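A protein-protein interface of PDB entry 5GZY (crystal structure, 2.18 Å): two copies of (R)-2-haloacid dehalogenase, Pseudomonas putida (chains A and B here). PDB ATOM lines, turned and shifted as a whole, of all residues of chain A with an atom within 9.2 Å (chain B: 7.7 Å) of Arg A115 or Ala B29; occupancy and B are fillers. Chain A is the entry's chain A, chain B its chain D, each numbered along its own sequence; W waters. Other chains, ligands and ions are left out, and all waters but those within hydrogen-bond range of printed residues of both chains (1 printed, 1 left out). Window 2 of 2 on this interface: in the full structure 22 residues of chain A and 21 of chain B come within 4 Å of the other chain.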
ATOM      1  N   GLY A 111      20.812 -29.150  27.567  1.00  0.00           N
ATOM      2  CA  GLY A 111      21.704 -28.141  27.029  1.00  0.00           C
ATOM      3  C   GLY A 111      22.431 -28.510  25.743  1.00  0.00           C
ATOM      4  O   GLY A 111      23.201 -27.708  25.217  1.00  0.00           O
ATOM      5  N   TYR A 112      22.199 -29.715  25.231  1.00  0.00           N
ATOM      6  CA  TYR A 112      22.824 -30.134  23.979  1.00  0.00           C
ATOM      7  C   TYR A 112      22.221 -29.403  22.786  1.00  0.00           C
ATOM      8  O   TYR A 112      21.008 -29.341  22.639  1.00  0.00           O
ATOM      9  CB  TYR A 112      22.686 -31.646  23.783  1.00  0.00           C
ATOM     10  CG  TYR A 112      23.622 -32.459  24.646  1.00  0.00           C
ATOM     11  CD1 TYR A 112      23.274 -32.816  25.946  1.00  0.00           C
ATOM     12  CD2 TYR A 112      24.860 -32.877  24.158  1.00  0.00           C
ATOM     13  CE1 TYR A 112      24.140 -33.554  26.736  1.00  0.00           C
ATOM     14  CE2 TYR A 112      25.715 -33.617  24.936  1.00  0.00           C
ATOM     15  CZ  TYR A 112      25.359 -33.951  26.223  1.00  0.00           C
ATOM     16  OH  TYR A 112      26.219 -34.692  27.001  1.00  0.00           O
ATOM     17  N   SER A 113      23.076 -28.859  21.934  1.00  0.00           N
ATOM     18  CA  SER A 113      22.625 -28.122  20.765  1.00  0.00           C
ATOM     19  C   SER A 113      22.346 -29.070  19.603  1.00  0.00           C
ATOM     20  O   SER A 113      22.629 -30.255  19.683  1.00  0.00           O
ATOM     21  CB  SER A 113      23.666 -27.077  20.351  1.00  0.00           C
ATOM     22  OG  SER A 113      24.819 -27.690  19.803  1.00  0.00           O
ATOM     23  N   VAL A 114      21.790 -28.528  18.528  1.00  0.00           N
ATOM     24  CA  VAL A 114      21.468 -29.307  17.341  1.00  0.00           C
ATOM     25  C   VAL A 114      22.733 -29.896  16.727  1.00  0.00           C
ATOM     26  O   VAL A 114      22.742 -31.048  16.335  1.00  0.00           O
ATOM     27  CB  VAL A 114      20.705 -28.435  16.300  1.00  0.00           C
ATOM     28  CG1 VAL A 114      20.768 -29.029  14.902  1.00  0.00           C
ATOM     29  CG2 VAL A 114      19.258 -28.242  16.741  1.00  0.00           C
ATOM     30  N   ARG A 115      23.810 -29.116  16.682  1.00  0.00           N
ATOM     31  CA  ARG A 115      25.068 -29.586  16.110  1.00  0.00           C
ATOM     32  C   ARG A 115      25.690 -30.709  16.931  1.00  0.00           C
ATOM     33  O   ARG A 115      26.229 -31.657  16.376  1.00  0.00           O
ATOM     34  CB  ARG A 115      26.078 -28.440  15.985  1.00  0.00           C
ATOM     35  CG  ARG A 115      25.733 -27.440  14.905  1.00  0.00           C
ATOM     36  CD  ARG A 115      26.910 -26.537  14.574  1.00  0.00           C
ATOM     37  NE  ARG A 115      26.532 -25.549  13.573  1.00  0.00           N
ATOM     38  CZ  ARG A 115      26.480 -24.235  13.782  1.00  0.00           C
ATOM     39  NH1 ARG A 115      26.795 -23.716  14.969  1.00  0.00           N
ATOM     40  NH2 ARG A 115      26.121 -23.432  12.785  1.00  0.00           N
ATOM     41  N   GLU A 116      25.620 -30.579  18.248  1.00  0.00           N
ATOM     42  CA  GLU A 116      26.197 -31.571  19.129  1.00  0.00           C
ATOM     43  C   GLU A 116      25.449 -32.903  18.989  1.00  0.00           C
ATOM     44  O   GLU A 116      26.063 -33.963  18.922  1.00  0.00           O
ATOM     45  CB  GLU A 116      26.169 -31.087  20.572  1.00  0.00           C
ATOM     46  CG  GLU A 116      27.131 -29.940  20.870  1.00  0.00           C
ATOM     47  CD  GLU A 116      27.068 -29.508  22.320  1.00  0.00           C
ATOM     48  OE1 GLU A 116      25.955 -29.507  22.878  1.00  0.00           O
ATOM     49  OE2 GLU A 116      28.126 -29.196  22.909  1.00  0.00           O
ATOM     50  N   ILE A 117      24.127 -32.839  18.913  1.00  0.00           N
ATOM     51  CA  ILE A 117      23.343 -34.050  18.767  1.00  0.00           C
ATOM     52  C   ILE A 117      23.668 -34.693  17.419  1.00  0.00           C
ATOM     53  O   ILE A 117      23.724 -35.907  17.314  1.00  0.00           O
ATOM     54  CB  ILE A 117      21.842 -33.777  18.902  1.00  0.00           C
ATOM     55  CG1 ILE A 117      21.556 -33.173  20.272  1.00  0.00           C
ATOM     56  CG2 ILE A 117      21.044 -35.067  18.747  1.00  0.00           C
ATOM     57  CD1 ILE A 117      20.131 -32.753  20.480  1.00  0.00           C
ATOM     58  N   GLY A 118      23.922 -33.867  16.410  1.00  0.00           N
ATOM     59  CA  GLY A 118      24.357 -34.352  15.117  1.00  0.00           C
ATOM     60  C   GLY A 118      25.682 -35.099  15.214  1.00  0.00           C
ATOM     61  O   GLY A 118      25.852 -36.155  14.607  1.00  0.00           O
ATOM     62  N   GLN A 119      26.620 -34.551  15.984  1.00  0.00           N
ATOM     63  CA  GLN A 119      27.906 -35.198  16.197  1.00  0.00           C
ATOM     64  C   GLN A 119      27.736 -36.542  16.909  1.00  0.00           C
ATOM     65  O   GLN A 119      28.402 -37.511  16.579  1.00  0.00           O
ATOM     66  CB  GLN A 119      28.836 -34.297  17.008  1.00  0.00           C
ATOM     67  CG  GLN A 119      29.313 -33.046  16.291  1.00  0.00           C
ATOM     68  CD  GLN A 119      30.044 -32.106  17.228  1.00  0.00           C
ATOM     69  OE1 GLN A 119      30.270 -32.425  18.389  1.00  0.00           O
ATOM     70  NE2 GLN A 119      30.425 -30.946  16.725  1.00  0.00           N
ATOM     71  N   ILE A 120      26.847 -36.583  17.890  1.00  0.00           N
ATOM     72  CA  ILE A 120      26.541 -37.815  18.607  1.00  0.00           C
ATOM     73  C   ILE A 120      26.004 -38.901  17.668  1.00  0.00           C
ATOM     74  O   ILE A 120      26.450 -40.049  17.712  1.00  0.00           O
ATOM     75  CB  ILE A 120      25.534 -37.553  19.750  1.00  0.00           C
ATOM     76  CG1 ILE A 120      26.205 -36.733  20.861  1.00  0.00           C
ATOM     77  CG2 ILE A 120      25.031 -38.858  20.331  1.00  0.00           C
ATOM     78  CD1 ILE A 120      25.254 -36.189  21.903  1.00  0.00           C
ATOM     79  N   ARG A 121      25.064 -38.526  16.807  1.00  0.00           N
ATOM     80  CA  ARG A 121      24.528 -39.443  15.805  1.00  0.00           C
ATOM     81  C   ARG A 121      25.629 -40.006  14.900  1.00  0.00           C
ATOM     82  O   ARG A 121      25.652 -41.191  14.610  1.00  0.00           O
ATOM     83  CB  ARG A 121      23.479 -38.749  14.952  1.00  0.00           C
ATOM     84  CG  ARG A 121      22.196 -38.417  15.666  1.00  0.00           C
ATOM     85  CD  ARG A 121      21.154 -37.939  14.678  1.00  0.00           C
ATOM     86  NE  ARG A 121      19.914 -37.555  15.341  1.00  0.00           N
ATOM     87  CZ  ARG A 121      19.497 -36.305  15.471  1.00  0.00           C
ATOM     88  NH1 ARG A 121      20.220 -35.310  14.968  1.00  0.00           N
ATOM     89  NH2 ARG A 121      18.357 -36.051  16.094  1.00  0.00           N
ATOM     90  N   ALA A 122      26.538 -39.134  14.472  1.00  0.00           N
ATOM     91  CA  ALA A 122      27.604 -39.503  13.558  1.00  0.00           C
ATOM     92  C   ALA A 122      28.522 -40.560  14.170  1.00  0.00           C
ATOM     93  O   ALA A 122      28.956 -41.471  13.483  1.00  0.00           O
ATOM     94  CB  ALA A 122      28.419 -38.262  13.151  1.00  0.00           C
ATOM     95  N   VAL A 123      28.815 -40.416  15.457  1.00  0.00           N
ATOM     96  CA  VAL A 123      29.592 -41.405  16.198  1.00  0.00           C
ATOM     97  C   VAL A 123      28.842 -42.744  16.255  1.00  0.00           C
ATOM     98  O   VAL A 123      29.428 -43.790  16.018  1.00  0.00           O
ATOM     99  CB  VAL A 123      29.911 -40.910  17.632  1.00  0.00           C
ATOM    100  CG1 VAL A 123      30.392 -42.047  18.503  1.00  0.00           C
ATOM    101  CG2 VAL A 123      30.953 -39.820  17.590  1.00  0.00           C
ATOM    102  N   TRP A 212      30.872 -37.636  25.757  1.00  0.00           N
ATOM    103  CA  TRP A 212      29.746 -36.894  26.316  1.00  0.00           C
ATOM    104  C   TRP A 212      29.133 -37.673  27.485  1.00  0.00           C
ATOM    105  O   TRP A 212      28.128 -38.355  27.319  1.00  0.00           O
ATOM    106  CB  TRP A 212      28.678 -36.650  25.256  1.00  0.00           C
ATOM    107  CG  TRP A 212      29.123 -35.929  24.026  1.00  0.00           C
ATOM    108  CD1 TRP A 212      29.267 -34.581  23.875  1.00  0.00           C
ATOM    109  CD2 TRP A 212      29.420 -36.506  22.753  1.00  0.00           C
ATOM    110  NE1 TRP A 212      29.660 -34.286  22.596  1.00  0.00           N
ATOM    111  CE2 TRP A 212      29.766 -35.456  21.881  1.00  0.00           C
ATOM    112  CE3 TRP A 212      29.451 -37.823  22.262  1.00  0.00           C
ATOM    113  CZ2 TRP A 212      30.125 -35.663  20.554  1.00  0.00           C
ATOM    114  CZ3 TRP A 212      29.807 -38.030  20.947  1.00  0.00           C
ATOM    115  CH2 TRP A 212      30.131 -36.957  20.107  1.00  0.00           C
ATOM    116  N   VAL B  24      28.297 -17.280  23.527  1.00  0.00           N
ATOM    117  CA  VAL B  24      27.733 -18.021  22.407  1.00  0.00           C
ATOM    118  C   VAL B  24      28.786 -18.984  21.884  1.00  0.00           C
ATOM    119  O   VAL B  24      29.721 -18.563  21.218  1.00  0.00           O
ATOM    120  CB  VAL B  24      27.272 -17.086  21.284  1.00  0.00           C
ATOM    121  CG1 VAL B  24      26.561 -17.855  20.198  1.00  0.00           C
ATOM    122  CG2 VAL B  24      26.387 -15.989  21.857  1.00  0.00           C
ATOM    123  N   PRO B  25      28.649 -20.283  22.209  1.00  0.00           N
ATOM    124  CA  PRO B  25      29.663 -21.265  21.812  1.00  0.00           C
ATOM    125  C   PRO B  25      29.629 -21.551  20.322  1.00  0.00           C
ATOM    126  O   PRO B  25      28.606 -21.325  19.681  1.00  0.00           O
ATOM    127  CB  PRO B  25      29.289 -22.515  22.618  1.00  0.00           C
ATOM    128  CG  PRO B  25      27.864 -22.360  22.931  1.00  0.00           C
ATOM    129  CD  PRO B  25      27.619 -20.880  23.075  1.00  0.00           C
ATOM    130  N   GLU B  26      30.735 -22.049  19.786  1.00  0.00           N
ATOM    131  CA  GLU B  26      30.835 -22.269  18.354  1.00  0.00           C
ATOM    132  C   GLU B  26      29.777 -23.251  17.866  1.00  0.00           C
ATOM    133  O   GLU B  26      29.280 -23.109  16.761  1.00  0.00           O
ATOM    134  CB  GLU B  26      32.234 -22.757  17.972  1.00  0.00           C
ATOM    135  CG  GLU B  26      33.361 -21.760  18.268  1.00  0.00           C
ATOM    136  CD  GLU B  26      34.701 -22.216  17.711  1.00  0.00           C
ATOM    137  OE1 GLU B  26      34.845 -22.285  16.479  1.00  0.00           O
ATOM    138  OE2 GLU B  26      35.607 -22.519  18.506  1.00  0.00           O
ATOM    139  N   HIS B  27      29.400 -24.222  18.692  1.00  0.00           N
ATOM    140  CA  HIS B  27      28.424 -25.206  18.248  1.00  0.00           C
ATOM    141  C   HIS B  27      26.986 -24.649  18.231  1.00  0.00           C
ATOM    142  O   HIS B  27      26.087 -25.302  17.714  1.00  0.00           O
ATOM    143  CB  HIS B  27      28.504 -26.485  19.104  1.00  0.00           C
ATOM    144  CG  HIS B  27      28.197 -26.282  20.561  1.00  0.00           C
ATOM    145  ND1 HIS B  27      26.924 -26.344  21.068  1.00  0.00           N
ATOM    146  CD2 HIS B  27      29.011 -26.031  21.614  1.00  0.00           C
ATOM    147  CE1 HIS B  27      26.957 -26.134  22.373  1.00  0.00           C
ATOM    148  NE2 HIS B  27      28.217 -25.940  22.727  1.00  0.00           N
ATOM    149  N   ARG B  28      26.778 -23.444  18.767  1.00  0.00           N
ATOM    150  CA  ARG B  28      25.455 -22.812  18.726  1.00  0.00           C
ATOM    151  C   ARG B  28      25.380 -21.584  17.816  1.00  0.00           C
ATOM    152  O   ARG B  28      24.295 -21.159  17.457  1.00  0.00           O
ATOM    153  CB  ARG B  28      25.001 -22.411  20.131  1.00  0.00           C
ATOM    154  CG  ARG B  28      24.697 -23.584  21.057  1.00  0.00           C
ATOM    155  CD  ARG B  28      24.155 -23.136  22.420  1.00  0.00           C
ATOM    156  NE  ARG B  28      24.010 -24.271  23.338  1.00  0.00           N
ATOM    157  CZ  ARG B  28      24.634 -24.364  24.516  1.00  0.00           C
ATOM    158  NH1 ARG B  28      25.417 -23.373  24.937  1.00  0.00           N
ATOM    159  NH2 ARG B  28      24.474 -25.432  25.289  1.00  0.00           N
ATOM    160  N   ALA B  29      26.521 -21.015  17.447  1.00  0.00           N
ATOM    161  CA  ALA B  29      26.549 -19.772  16.687  1.00  0.00           C
ATOM    162  C   ALA B  29      25.855 -19.888  15.335  1.00  0.00           C
ATOM    163  O   ALA B  29      26.087 -20.836  14.599  1.00  0.00           O
ATOM    164  CB  ALA B  29      27.991 -19.311  16.485  1.00  0.00           C
ATOM    165  N   ASP B  30      25.016 -18.913  15.002  1.00  0.00           N
ATOM    166  CA  ASP B  30      24.331 -18.936  13.721  1.00  0.00           C
ATOM    167  C   ASP B  30      25.318 -18.625  12.607  1.00  0.00           C
ATOM    168  O   ASP B  30      26.491 -18.371  12.859  1.00  0.00           O
ATOM    169  CB  ASP B  30      23.133 -17.960  13.703  1.00  0.00           C
ATOM    170  CG  ASP B  30      23.538 -16.486  13.896  1.00  0.00           C
ATOM    171  OD1 ASP B  30      24.689 -16.103  13.615  1.00  0.00           O
ATOM    172  OD2 ASP B  30      22.676 -15.699  14.330  1.00  0.00           O
ATOM    173  N   GLN B  31      24.826 -18.647  11.377  1.00  0.00           N
ATOM    174  CA  GLN B  31      25.634 -18.437  10.177  1.00  0.00           C
ATOM    175  C   GLN B  31      26.474 -17.156  10.209  1.00  0.00           C
ATOM    176  O   GLN B  31      27.671 -17.175   9.941  1.00  0.00           O
ATOM    177  CB  GLN B  31      24.710 -18.401   8.967  1.00  0.00           C
ATOM    178  CG  GLN B  31      25.361 -18.564   7.624  1.00  0.00           C
ATOM    179  CD  GLN B  31      24.342 -18.426   6.501  1.00  0.00           C
ATOM    180  OE1 GLN B  31      23.566 -17.470   6.458  1.00  0.00           O
ATOM    181  NE2 GLN B  31      24.307 -19.412   5.613  1.00  0.00           N
ATOM    182  N   GLU B  32      25.826 -16.045  10.526  1.00  0.00           N
ATOM    183  CA  GLU B  32      26.478 -14.744  10.515  1.00  0.00           C
ATOM    184  C   GLU B  32      27.556 -14.626  11.595  1.00  0.00           C
ATOM    185  O   GLU B  32      28.638 -14.100  11.340  1.00  0.00           O
ATOM    186  CB  GLU B  32      25.426 -13.646  10.674  1.00  0.00           C
ATOM    187  CG  GLU B  32      25.949 -12.275  11.066  1.00  0.00           C
ATOM    188  CD  GLU B  32      24.816 -11.308  11.378  1.00  0.00           C
ATOM    189  OE1 GLU B  32      24.593 -11.003  12.567  1.00  0.00           O
ATOM    190  OE2 GLU B  32      24.140 -10.866  10.427  1.00  0.00           O
ATOM    191  N   LEU B  33      27.268 -15.114  12.796  1.00  0.00           N
ATOM    192  CA  LEU B  33      28.254 -15.062  13.860  1.00  0.00           C
ATOM    193  C   LEU B  33      29.415 -15.994  13.530  1.00  0.00           C
ATOM    194  O   LEU B  33      30.570 -15.660  13.765  1.00  0.00           O
ATOM    195  CB  LEU B  33      27.634 -15.421  15.211  1.00  0.00           C
ATOM    196  CG  LEU B  33      28.566 -15.365  16.425  1.00  0.00           C
ATOM    197  CD1 LEU B  33      29.355 -14.057  16.468  1.00  0.00           C
ATOM    198  CD2 LEU B  33      27.786 -15.562  17.708  1.00  0.00           C
ATOM    199  N   SER B  34      29.102 -17.145  12.945  1.00  0.00           N
ATOM    200  CA  SER B  34      30.117 -18.133  12.603  1.00  0.00           C
ATOM    201  C   SER B  34      31.135 -17.603  11.605  1.00  0.00           C
ATOM    202  O   SER B  34      32.280 -18.025  11.618  1.00  0.00           O
ATOM    203  CB  SER B  34      29.470 -19.401  12.054  1.00  0.00           C
ATOM    204  OG  SER B  34      28.809 -20.111  13.079  1.00  0.00           O
ATOM    205  N   GLU B  35      30.721 -16.674  10.753  1.00  0.00           N
ATOM    206  CA  GLU B  35      31.640 -16.047   9.811  1.00  0.00           C
ATOM    207  C   GLU B  35      32.652 -15.154  10.526  1.00  0.00           C
ATOM    208  O   GLU B  35      33.837 -15.159  10.199  1.00  0.00           O
ATOM    209  CB  GLU B  35      30.870 -15.234   8.771  1.00  0.00           C
ATOM    210  CG  GLU B  35      31.748 -14.475   7.798  1.00  0.00           C
ATOM    211  CD  GLU B  35      32.854 -15.327   7.183  1.00  0.00           C
ATOM    212  OE1 GLU B  35      32.601 -16.515   6.862  1.00  0.00           O
ATOM    213  OE2 GLU B  35      33.979 -14.801   7.015  1.00  0.00           O
ATOM    214  N   TYR B  37      33.490 -15.474  13.726  1.00  0.00           N
ATOM    215  CA  TYR B  37      34.274 -16.493  14.420  1.00  0.00           C
ATOM    216  C   TYR B  37      35.361 -17.098  13.542  1.00  0.00           C
ATOM    217  O   TYR B  37      36.486 -17.317  13.997  1.00  0.00           O
ATOM    218  CB  TYR B  37      33.368 -17.610  14.935  1.00  0.00           C
ATOM    219  CG  TYR B  37      32.664 -17.294  16.231  1.00  0.00           C
ATOM    220  CD1 TYR B  37      32.793 -16.052  16.833  1.00  0.00           C
ATOM    221  CD2 TYR B  37      31.888 -18.244  16.860  1.00  0.00           C
ATOM    222  CE1 TYR B  37      32.157 -15.769  18.017  1.00  0.00           C
ATOM    223  CE2 TYR B  37      31.252 -17.971  18.033  1.00  0.00           C
ATOM    224  CZ  TYR B  37      31.385 -16.738  18.609  1.00  0.00           C
ATOM    225  OH  TYR B  37      30.748 -16.478  19.782  1.00  0.00           O
ATOM    226  N   ALA B  57      30.495 -11.658  22.104  1.00  0.00           N
ATOM    227  CA  ALA B  57      29.619 -11.898  20.955  1.00  0.00           C
ATOM    228  C   ALA B  57      28.127 -11.809  21.304  1.00  0.00           C
ATOM    229  O   ALA B  57      27.309 -11.552  20.437  1.00  0.00           O
ATOM    230  CB  ALA B  57      29.929 -13.250  20.327  1.00  0.00           C
ATOM    231  N   ARG B  60      26.316  -8.567  20.022  1.00  0.00           N
ATOM    232  CA  ARG B  60      26.858  -8.857  18.699  1.00  0.00           C
ATOM    233  C   ARG B  60      27.284  -7.639  17.871  1.00  0.00           C
ATOM    234  O   ARG B  60      28.339  -7.688  17.247  1.00  0.00           O
ATOM    235  CB  ARG B  60      25.880  -9.696  17.867  1.00  0.00           C
ATOM    236  CG  ARG B  60      26.598 -10.383  16.701  1.00  0.00           C
ATOM    237  CD  ARG B  60      25.674 -11.142  15.796  1.00  0.00           C
ATOM    238  NE  ARG B  60      25.101 -12.308  16.445  1.00  0.00           N
ATOM    239  CZ  ARG B  60      24.428 -13.259  15.808  1.00  0.00           C
ATOM    240  NH1 ARG B  60      24.255 -13.183  14.492  1.00  0.00           N
ATOM    241  NH2 ARG B  60      23.931 -14.284  16.485  1.00  0.00           N
HETATM  242  O   HOH W   1      23.525 -26.194  17.110  1.00  0.00           O
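NH1 of Arg A115 sits at hydrogen-bond distance from O of Glu B26, 3.1 Å away. O of Ala B29 is in hydrogen-bond range of NH1 of Arg A115, at 3.0 Å. The side-chain hydroxyl (OG) of Ser A113 is in hydrogen-bond range of a ring nitrogen (ND1) of His B27. OE2 of Glu A116 sits at hydrogen-bond distance from NE2 of His B27 (3.3 Å). The backbone carbonyl oxygen (O) of Gly A111 lies within hydrogen-bond range of the guanidinium group (NH2) of Arg B28, at 2.6 Å. The backbone carbonyl oxygen of His B27 sits at hydrogen-bond distance from the guanidinium group of Arg A115 (3.2 Å).
The backbone carbonyl oxygen (O) of Ala B29 sits at hydrogen-bond distance from the side-chain hydroxyl (OG) of Ser B34 (3.2 Å). The side-chain carboxylate of Glu A116 is in hydrogen-bond range of the backbone NH of Ser A113, at 3.1 Å.
Ser A113 touches Arg B28 (CB to CG, 3.7 Å). Arg A115 touches Arg B28.
Arg A115 touches just these residues of chain B: Glu B26, His B27, Arg B28 and Ala B29. Ala B29 touches one residue of chain A. Printed residues of chain B within 4 Å of Gly A111: Arg B28 (2.6 Å). Printed residues of chain A within 4 Å of Glu B26: Arg A115 (3.1 Å). Val B24 touches none of the printed residues of chain A. Ser B34 touches none of the printed residues of chain A. The nearest printed residue of chain A that does not touch His B27 is Gly A111 (5.0 Å).
Among the printed residues, no Asp or Glu carboxylate lies within 4 Å of a Lys or Arg side-chain nitrogen of the other chain.
No position is printed for both chains. Of the 8 pairs that touch across the chains among the printed residues, none has its exchanged pair printed and touching as well.
Water W1 lies within hydrogen-bond range of O of His B27 (2.8 Å), N of Arg A115 (3.0 Å), N of Val A114 (3.2 Å) and OG of Ser A113 (3.3 Å).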
